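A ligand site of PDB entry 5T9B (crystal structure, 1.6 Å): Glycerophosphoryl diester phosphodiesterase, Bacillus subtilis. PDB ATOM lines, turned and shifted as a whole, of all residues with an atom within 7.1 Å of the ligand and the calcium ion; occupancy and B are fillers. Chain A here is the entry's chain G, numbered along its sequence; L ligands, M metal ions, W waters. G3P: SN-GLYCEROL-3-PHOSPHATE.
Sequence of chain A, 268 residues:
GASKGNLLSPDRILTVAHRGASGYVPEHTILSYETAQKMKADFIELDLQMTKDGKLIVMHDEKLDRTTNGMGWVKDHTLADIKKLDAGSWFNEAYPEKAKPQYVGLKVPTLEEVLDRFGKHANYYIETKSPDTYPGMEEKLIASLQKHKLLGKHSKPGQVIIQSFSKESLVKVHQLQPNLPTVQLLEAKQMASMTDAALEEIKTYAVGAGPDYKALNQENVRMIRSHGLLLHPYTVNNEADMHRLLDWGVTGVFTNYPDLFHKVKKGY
The side-chain amide oxygen (OE1) of Gln 163 lies close to an oxygen (O1) of the ligand, 2.7 Å away. O2P of the ligand sits at hydrogen-bond distance from NE2 of His 60 (2.8 Å). O4P of the ligand is in salt-bridge range of NH2 of Arg 19, at 2.8 Å. O4P of the ligand lies within hydrogen-bond range of NE2 of His 18 (2.8 Å).
The backbone carbonyl oxygen (O) of Tyr 125 lies within hydrogen-bond range of the side-chain amide nitrogen (NE2) of Gln 163 (3.5 Å). NE2 of His 18 sits close to OG1 of Thr 235 (3.3 Å). NH2 of Arg 19 sits at hydrogen-bond distance from NE2 of His 60, at 3.2 Å. OD2 of Asp 47 lies within hydrogen-bond range of NE2 of His 28, at 2.7 Å. The side-chain carboxylate of Glu 45 sits at hydrogen-bond distance from the backbone NH of Arg 19 (2.9 Å). The backbone carbonyl oxygen (O) of Leu 46 lies within hydrogen-bond range of the backbone NH (N) of Glu 127. The backbone NH (N) of Phe 254 sits at hydrogen-bond distance from the backbone carbonyl oxygen (O) of Pro 233, at 2.9 Å. The side-chain amide nitrogen (NE2) of Gln 163 sits close to the side-chain carboxylate (OE2) of Glu 45, 2.8 Å away.
Merely in contact with the ligand: Leu 185 (3.4 Å), Tyr 234 (3.3 Å) and Phe 254 (3.7 Å). Hydrophobic or aromatic side chains that line the ligand: His 18, His 60, Leu 185, Tyr 234 and Phe 254. Nine residues have an atom within 4 Å of the ligand: His 18, Arg 19, Glu 45, His 60, Glu 127, Gln 163, Leu 185, Tyr 234 and Phe 254. The nearest printed residue that does not touch the ligand is Phe 165 (4.1 Å).
Merely in contact with the calcium ion: Gln 163 (3.9 Å). The nearest printed residue that does not touch the calcium ion is His 18 (4.7 Å).
The calcium ion is bound by an oxygen (O2) of the ligand (2.1 Å), the side-chain carboxylate (OE2) of Glu 45 (2.3 Å), water W5 (2.3 Å), the side-chain carboxylate (OE1) of Glu 127 (2.3 Å), the side-chain carboxylate (OD1) of Asp 47 (2.4 Å), an oxygen (O1) of the ligand (2.5 Å) and water W3 (2.6 Å). The calcium ion has seven donor atoms within binding distance.
Water W3 lies within hydrogen-bond range of the side-chain carboxylate of Asp 47 (2.6 Å), the side-chain carboxylate of Glu 45 (2.8 Å), the guanidinium group of Arg 19 (3.1 Å), a ring nitrogen (NE2) of His 18 (3.2 Å) and an oxygen (O4P) of the ligand (3.5 Å). Water W5 lies within hydrogen-bond range of O2P of the ligand (2.8 Å), NE2 of His 60 (3.4 Å) and OE2 of Glu 127 (3.4 Å). Water W4 lies within hydrogen-bond range of an oxygen (O3P) of the ligand (2.7 Å) and the guanidinium group (NH2) of Arg 19 (3.1 Å). Water W6 bridges the side-chain hydroxyl (OG1) of Thr 235 and an oxygen (O3P) of the ligand.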
ATOM      1  N   HIS A  18     -33.081 -11.635  20.084  1.00  0.00           N
ATOM      2  CA  HIS A  18     -31.714 -11.920  19.655  1.00  0.00           C
ATOM      3  C   HIS A  18     -30.835 -10.674  19.753  1.00  0.00           C
ATOM      4  O   HIS A  18     -30.956  -9.755  18.959  1.00  0.00           O
ATOM      5  CB  HIS A  18     -31.776 -12.441  18.223  1.00  0.00           C
ATOM      6  CG  HIS A  18     -30.463 -12.885  17.656  1.00  0.00           C
ATOM      7  ND1 HIS A  18     -29.936 -12.363  16.503  1.00  0.00           N
ATOM      8  CD2 HIS A  18     -29.602 -13.864  18.059  1.00  0.00           C
ATOM      9  CE1 HIS A  18     -28.795 -12.965  16.222  1.00  0.00           C
ATOM     10  NE2 HIS A  18     -28.578 -13.886  17.146  1.00  0.00           N
ATOM     11  N   ARG A  19     -29.945 -10.658  20.731  1.00  0.00           N
ATOM     12  CA  ARG A  19     -29.139  -9.471  20.992  1.00  0.00           C
ATOM     13  C   ARG A  19     -30.012  -8.231  21.284  1.00  0.00           C
ATOM     14  O   ARG A  19     -29.620  -7.098  21.020  1.00  0.00           O
ATOM     15  CB  ARG A  19     -28.174  -9.205  19.811  1.00  0.00           C
ATOM     16  CG  ARG A  19     -27.583 -10.459  19.221  1.00  0.00           C
ATOM     17  CD  ARG A  19     -26.534 -10.181  18.179  1.00  0.00           C
ATOM     18  NE  ARG A  19     -26.196 -11.405  17.462  1.00  0.00           N
ATOM     19  CZ  ARG A  19     -25.576 -11.453  16.293  1.00  0.00           C
ATOM     20  NH1 ARG A  19     -25.216 -10.331  15.684  1.00  0.00           N
ATOM     21  NH2 ARG A  19     -25.366 -12.620  15.710  1.00  0.00           N
ATOM     22  N   HIS A  28     -26.947  -5.700  21.488  1.00  0.00           N
ATOM     23  CA  HIS A  28     -26.218  -5.821  22.753  1.00  0.00           C
ATOM     24  C   HIS A  28     -25.881  -4.469  23.359  1.00  0.00           C
ATOM     25  O   HIS A  28     -24.740  -4.220  23.801  1.00  0.00           O
ATOM     26  CB  HIS A  28     -24.952  -6.668  22.547  1.00  0.00           C
ATOM     27  CG  HIS A  28     -25.217  -8.118  22.289  1.00  0.00           C
ATOM     28  ND1 HIS A  28     -26.202  -8.830  22.941  1.00  0.00           N
ATOM     29  CD2 HIS A  28     -24.591  -9.006  21.474  1.00  0.00           C
ATOM     30  CE1 HIS A  28     -26.177 -10.089  22.543  1.00  0.00           C
ATOM     31  NE2 HIS A  28     -25.203 -10.226  21.658  1.00  0.00           N
ATOM     32  N   GLU A  45     -31.491 -11.637  25.014  1.00  0.00           N
ATOM     33  CA  GLU A  45     -30.417 -12.583  24.718  1.00  0.00           C
ATOM     34  C   GLU A  45     -29.039 -11.918  24.726  1.00  0.00           C
ATOM     35  O   GLU A  45     -28.824 -10.898  24.067  1.00  0.00           O
ATOM     36  CB  GLU A  45     -30.678 -13.266  23.357  1.00  0.00           C
ATOM     37  CG  GLU A  45     -29.791 -14.489  23.104  1.00  0.00           C
ATOM     38  CD  GLU A  45     -28.750 -14.285  22.009  1.00  0.00           C
ATOM     39  OE1 GLU A  45     -28.753 -13.212  21.350  1.00  0.00           O
ATOM     40  OE2 GLU A  45     -27.940 -15.204  21.809  1.00  0.00           O
ATOM     41  N   LEU A  46     -28.132 -12.507  25.505  1.00  0.00           N
ATOM     42  CA  LEU A  46     -26.788 -11.968  25.741  1.00  0.00           C
ATOM     43  C   LEU A  46     -25.704 -12.944  25.252  1.00  0.00           C
ATOM     44  O   LEU A  46     -25.799 -14.149  25.488  1.00  0.00           O
ATOM     45  CB  LEU A  46     -26.591 -11.706  27.239  1.00  0.00           C
ATOM     46  CG  LEU A  46     -27.224 -10.493  27.909  1.00  0.00           C
ATOM     47  CD1 LEU A  46     -28.740 -10.471  27.879  1.00  0.00           C
ATOM     48  CD2 LEU A  46     -26.749 -10.439  29.369  1.00  0.00           C
ATOM     49  N   ASP A  47     -24.672 -12.415  24.588  1.00  0.00           N
ATOM     50  CA  ASP A  47     -23.459 -13.171  24.259  1.00  0.00           C
ATOM     51  C   ASP A  47     -22.337 -12.618  25.130  1.00  0.00           C
ATOM     52  O   ASP A  47     -22.172 -11.410  25.165  1.00  0.00           O
ATOM     53  CB  ASP A  47     -23.059 -13.054  22.788  1.00  0.00           C
ATOM     54  CG  ASP A  47     -24.159 -13.496  21.834  1.00  0.00           C
ATOM     55  OD1 ASP A  47     -24.709 -14.615  21.983  1.00  0.00           O
ATOM     56  OD2 ASP A  47     -24.452 -12.706  20.909  1.00  0.00           O
ATOM     57  N   HIS A  60     -21.191  -9.991  20.630  1.00  0.00           N
ATOM     58  CA  HIS A  60     -21.345 -11.219  19.879  1.00  0.00           C
ATOM     59  C   HIS A  60     -20.002 -11.772  19.389  1.00  0.00           C
ATOM     60  O   HIS A  60     -19.723 -12.962  19.536  1.00  0.00           O
ATOM     61  CB  HIS A  60     -22.274 -11.028  18.676  1.00  0.00           C
ATOM     62  CG  HIS A  60     -22.388 -12.245  17.821  1.00  0.00           C
ATOM     63  ND1 HIS A  60     -21.611 -12.439  16.701  1.00  0.00           N
ATOM     64  CD2 HIS A  60     -23.117 -13.380  17.969  1.00  0.00           C
ATOM     65  CE1 HIS A  60     -21.890 -13.614  16.162  1.00  0.00           C
ATOM     66  NE2 HIS A  60     -22.806 -14.197  16.903  1.00  0.00           N
ATOM     67  N   TYR A 125     -31.239 -14.833  28.497  1.00  0.00           N
ATOM     68  CA  TYR A 125     -30.838 -15.980  27.691  1.00  0.00           C
ATOM     69  C   TYR A 125     -29.360 -15.780  27.360  1.00  0.00           C
ATOM     70  O   TYR A 125     -29.020 -15.014  26.468  1.00  0.00           O
ATOM     71  CB  TYR A 125     -31.710 -16.072  26.423  1.00  0.00           C
ATOM     72  CG  TYR A 125     -32.031 -17.455  25.888  1.00  0.00           C
ATOM     73  CD1 TYR A 125     -31.027 -18.319  25.459  1.00  0.00           C
ATOM     74  CD2 TYR A 125     -33.354 -17.861  25.741  1.00  0.00           C
ATOM     75  CE1 TYR A 125     -31.330 -19.565  24.934  1.00  0.00           C
ATOM     76  CE2 TYR A 125     -33.674 -19.108  25.218  1.00  0.00           C
ATOM     77  CZ  TYR A 125     -32.664 -19.950  24.808  1.00  0.00           C
ATOM     78  OH  TYR A 125     -32.973 -21.175  24.287  1.00  0.00           O
ATOM     79  N   ILE A 126     -28.475 -16.435  28.125  1.00  0.00           N
ATOM     80  CA  ILE A 126     -27.058 -16.036  28.175  1.00  0.00           C
ATOM     81  C   ILE A 126     -26.098 -17.080  27.588  1.00  0.00           C
ATOM     82  O   ILE A 126     -26.100 -18.236  28.005  1.00  0.00           O
ATOM     83  CB  ILE A 126     -26.636 -15.723  29.630  1.00  0.00           C
ATOM     84  CG1 ILE A 126     -27.575 -14.691  30.240  1.00  0.00           C
ATOM     85  CG2 ILE A 126     -25.197 -15.217  29.652  1.00  0.00           C
ATOM     86  CD1 ILE A 126     -27.258 -14.388  31.736  1.00  0.00           C
ATOM     87  N   GLU A 127     -25.286 -16.655  26.620  1.00  0.00           N
ATOM     88  CA  GLU A 127     -24.424 -17.604  25.911  1.00  0.00           C
ATOM     89  C   GLU A 127     -22.996 -17.661  26.462  1.00  0.00           C
ATOM     90  O   GLU A 127     -22.342 -16.643  26.592  1.00  0.00           O
ATOM     91  CB  GLU A 127     -24.338 -17.262  24.428  1.00  0.00           C
ATOM     92  CG  GLU A 127     -23.629 -18.323  23.609  1.00  0.00           C
ATOM     93  CD  GLU A 127     -23.855 -18.160  22.124  1.00  0.00           C
ATOM     94  OE1 GLU A 127     -24.938 -17.660  21.721  1.00  0.00           O
ATOM     95  OE2 GLU A 127     -22.947 -18.514  21.344  1.00  0.00           O
ATOM     96  N   GLN A 163     -27.123 -20.860  27.295  1.00  0.00           N
ATOM     97  CA  GLN A 163     -26.993 -21.472  25.983  1.00  0.00           C
ATOM     98  C   GLN A 163     -25.549 -21.512  25.557  1.00  0.00           C
ATOM     99  O   GLN A 163     -24.757 -20.673  25.970  1.00  0.00           O
ATOM    100  CB  GLN A 163     -27.820 -20.678  24.954  1.00  0.00           C
ATOM    101  CG  GLN A 163     -27.467 -19.190  25.012  1.00  0.00           C
ATOM    102  CD  GLN A 163     -27.958 -18.417  23.808  1.00  0.00           C
ATOM    103  OE1 GLN A 163     -28.370 -19.004  22.811  1.00  0.00           O
ATOM    104  NE2 GLN A 163     -27.914 -17.098  23.900  1.00  0.00           N
ATOM    105  N   SER A 164     -25.182 -22.485  24.725  1.00  0.00           N
ATOM    106  CA  SER A 164     -23.832 -22.544  24.183  1.00  0.00           C
ATOM    107  C   SER A 164     -23.758 -23.527  23.008  1.00  0.00           C
ATOM    108  O   SER A 164     -24.510 -24.502  22.960  1.00  0.00           O
ATOM    109  CB  SER A 164     -22.829 -22.964  25.276  1.00  0.00           C
ATOM    110  OG  SER A 164     -21.499 -22.943  24.785  1.00  0.00           O
ATOM    111  N   PHE A 165     -22.861 -23.259  22.060  1.00  0.00           N
ATOM    112  CA  PHE A 165     -22.525 -24.257  21.043  1.00  0.00           C
ATOM    113  C   PHE A 165     -21.655 -25.353  21.648  1.00  0.00           C
ATOM    114  O   PHE A 165     -21.521 -26.451  21.086  1.00  0.00           O
ATOM    115  CB  PHE A 165     -21.804 -23.613  19.854  1.00  0.00           C
ATOM    116  CG  PHE A 165     -22.693 -22.809  18.958  1.00  0.00           C
ATOM    117  CD1 PHE A 165     -23.287 -23.397  17.841  1.00  0.00           C
ATOM    118  CD2 PHE A 165     -22.930 -21.469  19.202  1.00  0.00           C
ATOM    119  CE1 PHE A 165     -24.114 -22.651  17.003  1.00  0.00           C
ATOM    120  CE2 PHE A 165     -23.750 -20.722  18.372  1.00  0.00           C
ATOM    121  CZ  PHE A 165     -24.343 -21.317  17.267  1.00  0.00           C
ATOM    122  N   LEU A 185     -26.952 -25.184  21.540  1.00  0.00           N
ATOM    123  CA  LEU A 185     -26.981 -24.548  20.238  1.00  0.00           C
ATOM    124  C   LEU A 185     -26.356 -25.476  19.187  1.00  0.00           C
ATOM    125  O   LEU A 185     -25.372 -26.158  19.454  1.00  0.00           O
ATOM    126  CB  LEU A 185     -26.246 -23.212  20.281  1.00  0.00           C
ATOM    127  CG  LEU A 185     -26.826 -22.186  21.256  1.00  0.00           C
ATOM    128  CD1 LEU A 185     -25.972 -20.922  21.294  1.00  0.00           C
ATOM    129  CD2 LEU A 185     -28.282 -21.852  20.890  1.00  0.00           C
ATOM    130  N   GLY A 210     -31.237 -25.341  20.279  1.00  0.00           N
ATOM    131  CA  GLY A 210     -31.320 -24.130  19.477  1.00  0.00           C
ATOM    132  C   GLY A 210     -30.562 -24.235  18.165  1.00  0.00           C
ATOM    133  O   GLY A 210     -29.396 -23.833  18.090  1.00  0.00           O
ATOM    134  N   HIS A 232     -35.870 -23.820  20.047  1.00  0.00           N
ATOM    135  CA  HIS A 232     -35.768 -22.390  19.757  1.00  0.00           C
ATOM    136  C   HIS A 232     -34.792 -22.142  18.620  1.00  0.00           C
ATOM    137  O   HIS A 232     -33.601 -21.929  18.861  1.00  0.00           O
ATOM    138  CB  HIS A 232     -35.286 -21.610  20.995  1.00  0.00           C
ATOM    139  CG  HIS A 232     -36.139 -21.798  22.218  1.00  0.00           C
ATOM    140  ND1 HIS A 232     -35.657 -21.569  23.495  1.00  0.00           N
ATOM    141  CD2 HIS A 232     -37.438 -22.153  22.366  1.00  0.00           C
ATOM    142  CE1 HIS A 232     -36.615 -21.800  24.373  1.00  0.00           C
ATOM    143  NE2 HIS A 232     -37.706 -22.157  23.710  1.00  0.00           N
ATOM    144  N   PRO A 233     -35.262 -22.192  17.369  1.00  0.00           N
ATOM    145  CA  PRO A 233     -34.329 -21.916  16.269  1.00  0.00           C
ATOM    146  C   PRO A 233     -33.905 -20.461  16.173  1.00  0.00           C
ATOM    147  O   PRO A 233     -34.617 -19.560  16.623  1.00  0.00           O
ATOM    148  CB  PRO A 233     -35.126 -22.316  15.019  1.00  0.00           C
ATOM    149  CG  PRO A 233     -36.550 -22.239  15.436  1.00  0.00           C
ATOM    150  CD  PRO A 233     -36.599 -22.574  16.886  1.00  0.00           C
ATOM    151  N   TYR A 234     -32.728 -20.247  15.585  1.00  0.00           N
ATOM    152  CA  TYR A 234     -32.195 -18.922  15.312  1.00  0.00           C
ATOM    153  C   TYR A 234     -31.811 -18.834  13.845  1.00  0.00           C
ATOM    154  O   TYR A 234     -31.642 -19.871  13.205  1.00  0.00           O
ATOM    155  CB  TYR A 234     -30.960 -18.668  16.192  1.00  0.00           C
ATOM    156  CG  TYR A 234     -29.795 -19.550  15.797  1.00  0.00           C
ATOM    157  CD1 TYR A 234     -28.916 -19.181  14.775  1.00  0.00           C
ATOM    158  CD2 TYR A 234     -29.560 -20.761  16.451  1.00  0.00           C
ATOM    159  CE1 TYR A 234     -27.869 -19.998  14.397  1.00  0.00           C
ATOM    160  CE2 TYR A 234     -28.511 -21.592  16.073  1.00  0.00           C
ATOM    161  CZ  TYR A 234     -27.663 -21.189  15.049  1.00  0.00           C
ATOM    162  OH  TYR A 234     -26.616 -22.006  14.670  1.00  0.00           O
ATOM    163  N   THR A 235     -31.705 -17.630  13.278  1.00  0.00           N
ATOM    164  CA  THR A 235     -32.301 -16.415  13.809  1.00  0.00           C
ATOM    165  C   THR A 235     -33.495 -16.123  12.883  1.00  0.00           C
ATOM    166  O   THR A 235     -33.309 -15.904  11.684  1.00  0.00           O
ATOM    167  CB  THR A 235     -31.313 -15.223  13.816  1.00  0.00           C
ATOM    168  OG1 THR A 235     -30.252 -15.500  14.751  1.00  0.00           O
ATOM    169  CG2 THR A 235     -32.012 -13.934  14.230  1.00  0.00           C
ATOM    170  N   PHE A 254     -35.276 -17.366  18.373  1.00  0.00           N
ATOM    171  CA  PHE A 254     -34.446 -16.177  18.479  1.00  0.00           C
ATOM    172  C   PHE A 254     -34.776 -15.267  17.309  1.00  0.00           C
ATOM    173  O   PHE A 254     -34.700 -15.710  16.161  1.00  0.00           O
ATOM    174  CB  PHE A 254     -32.953 -16.494  18.450  1.00  0.00           C
ATOM    175  CG  PHE A 254     -32.481 -17.409  19.535  1.00  0.00           C
ATOM    176  CD1 PHE A 254     -32.649 -18.790  19.452  1.00  0.00           C
ATOM    177  CD2 PHE A 254     -31.787 -16.895  20.626  1.00  0.00           C
ATOM    178  CE1 PHE A 254     -32.179 -19.632  20.439  1.00  0.00           C
ATOM    179  CE2 PHE A 254     -31.311 -17.736  21.621  1.00  0.00           C
ATOM    180  CZ  PHE A 254     -31.509 -19.097  21.536  1.00  0.00           C
HETATM  181  O1  G3P L   1     -27.482 -18.044  20.403  1.00  0.00           O
HETATM  182  C1  G3P L   1     -28.419 -18.053  19.306  1.00  0.00           C
HETATM  183  C2  G3P L   1     -27.806 -17.189  18.245  1.00  0.00           C
HETATM  184  O2  G3P L   1     -27.331 -15.999  18.878  1.00  0.00           O
HETATM  185  C3  G3P L   1     -26.684 -18.014  17.629  1.00  0.00           C
HETATM  186  O1P G3P L   1     -26.438 -17.671  16.285  1.00  0.00           O
HETATM  187  O4P G3P L   1     -26.212 -15.134  16.463  1.00  0.00           O
HETATM  188  O2P G3P L   1     -24.193 -16.582  16.531  1.00  0.00           O
HETATM  189  O3P G3P L   1     -25.442 -16.268  14.409  1.00  0.00           O
HETATM  190  P   G3P L   1     -25.565 -16.391  15.905  1.00  0.00           P
HETATM  191 CA    CA M   1     -26.095 -15.951  20.603  1.00  0.00          CA
HETATM  192  O   HOH W   1     -24.932 -18.243  12.502  1.00  0.00           O
HETATM  193  O   HOH W   2     -21.890 -17.877  15.680  1.00  0.00           O
HETATM  194  O   HOH W   3     -26.557 -13.628  19.603  1.00  0.00           O
HETATM  195  O   HOH W   4     -24.198 -14.189  13.333  1.00  0.00           O
HETATM  196  O   HOH W   5     -24.185 -16.127  19.272  1.00  0.00           O
HETATM  197  O   HOH W   6     -27.930 -15.776  13.267  1.00  0.00           O
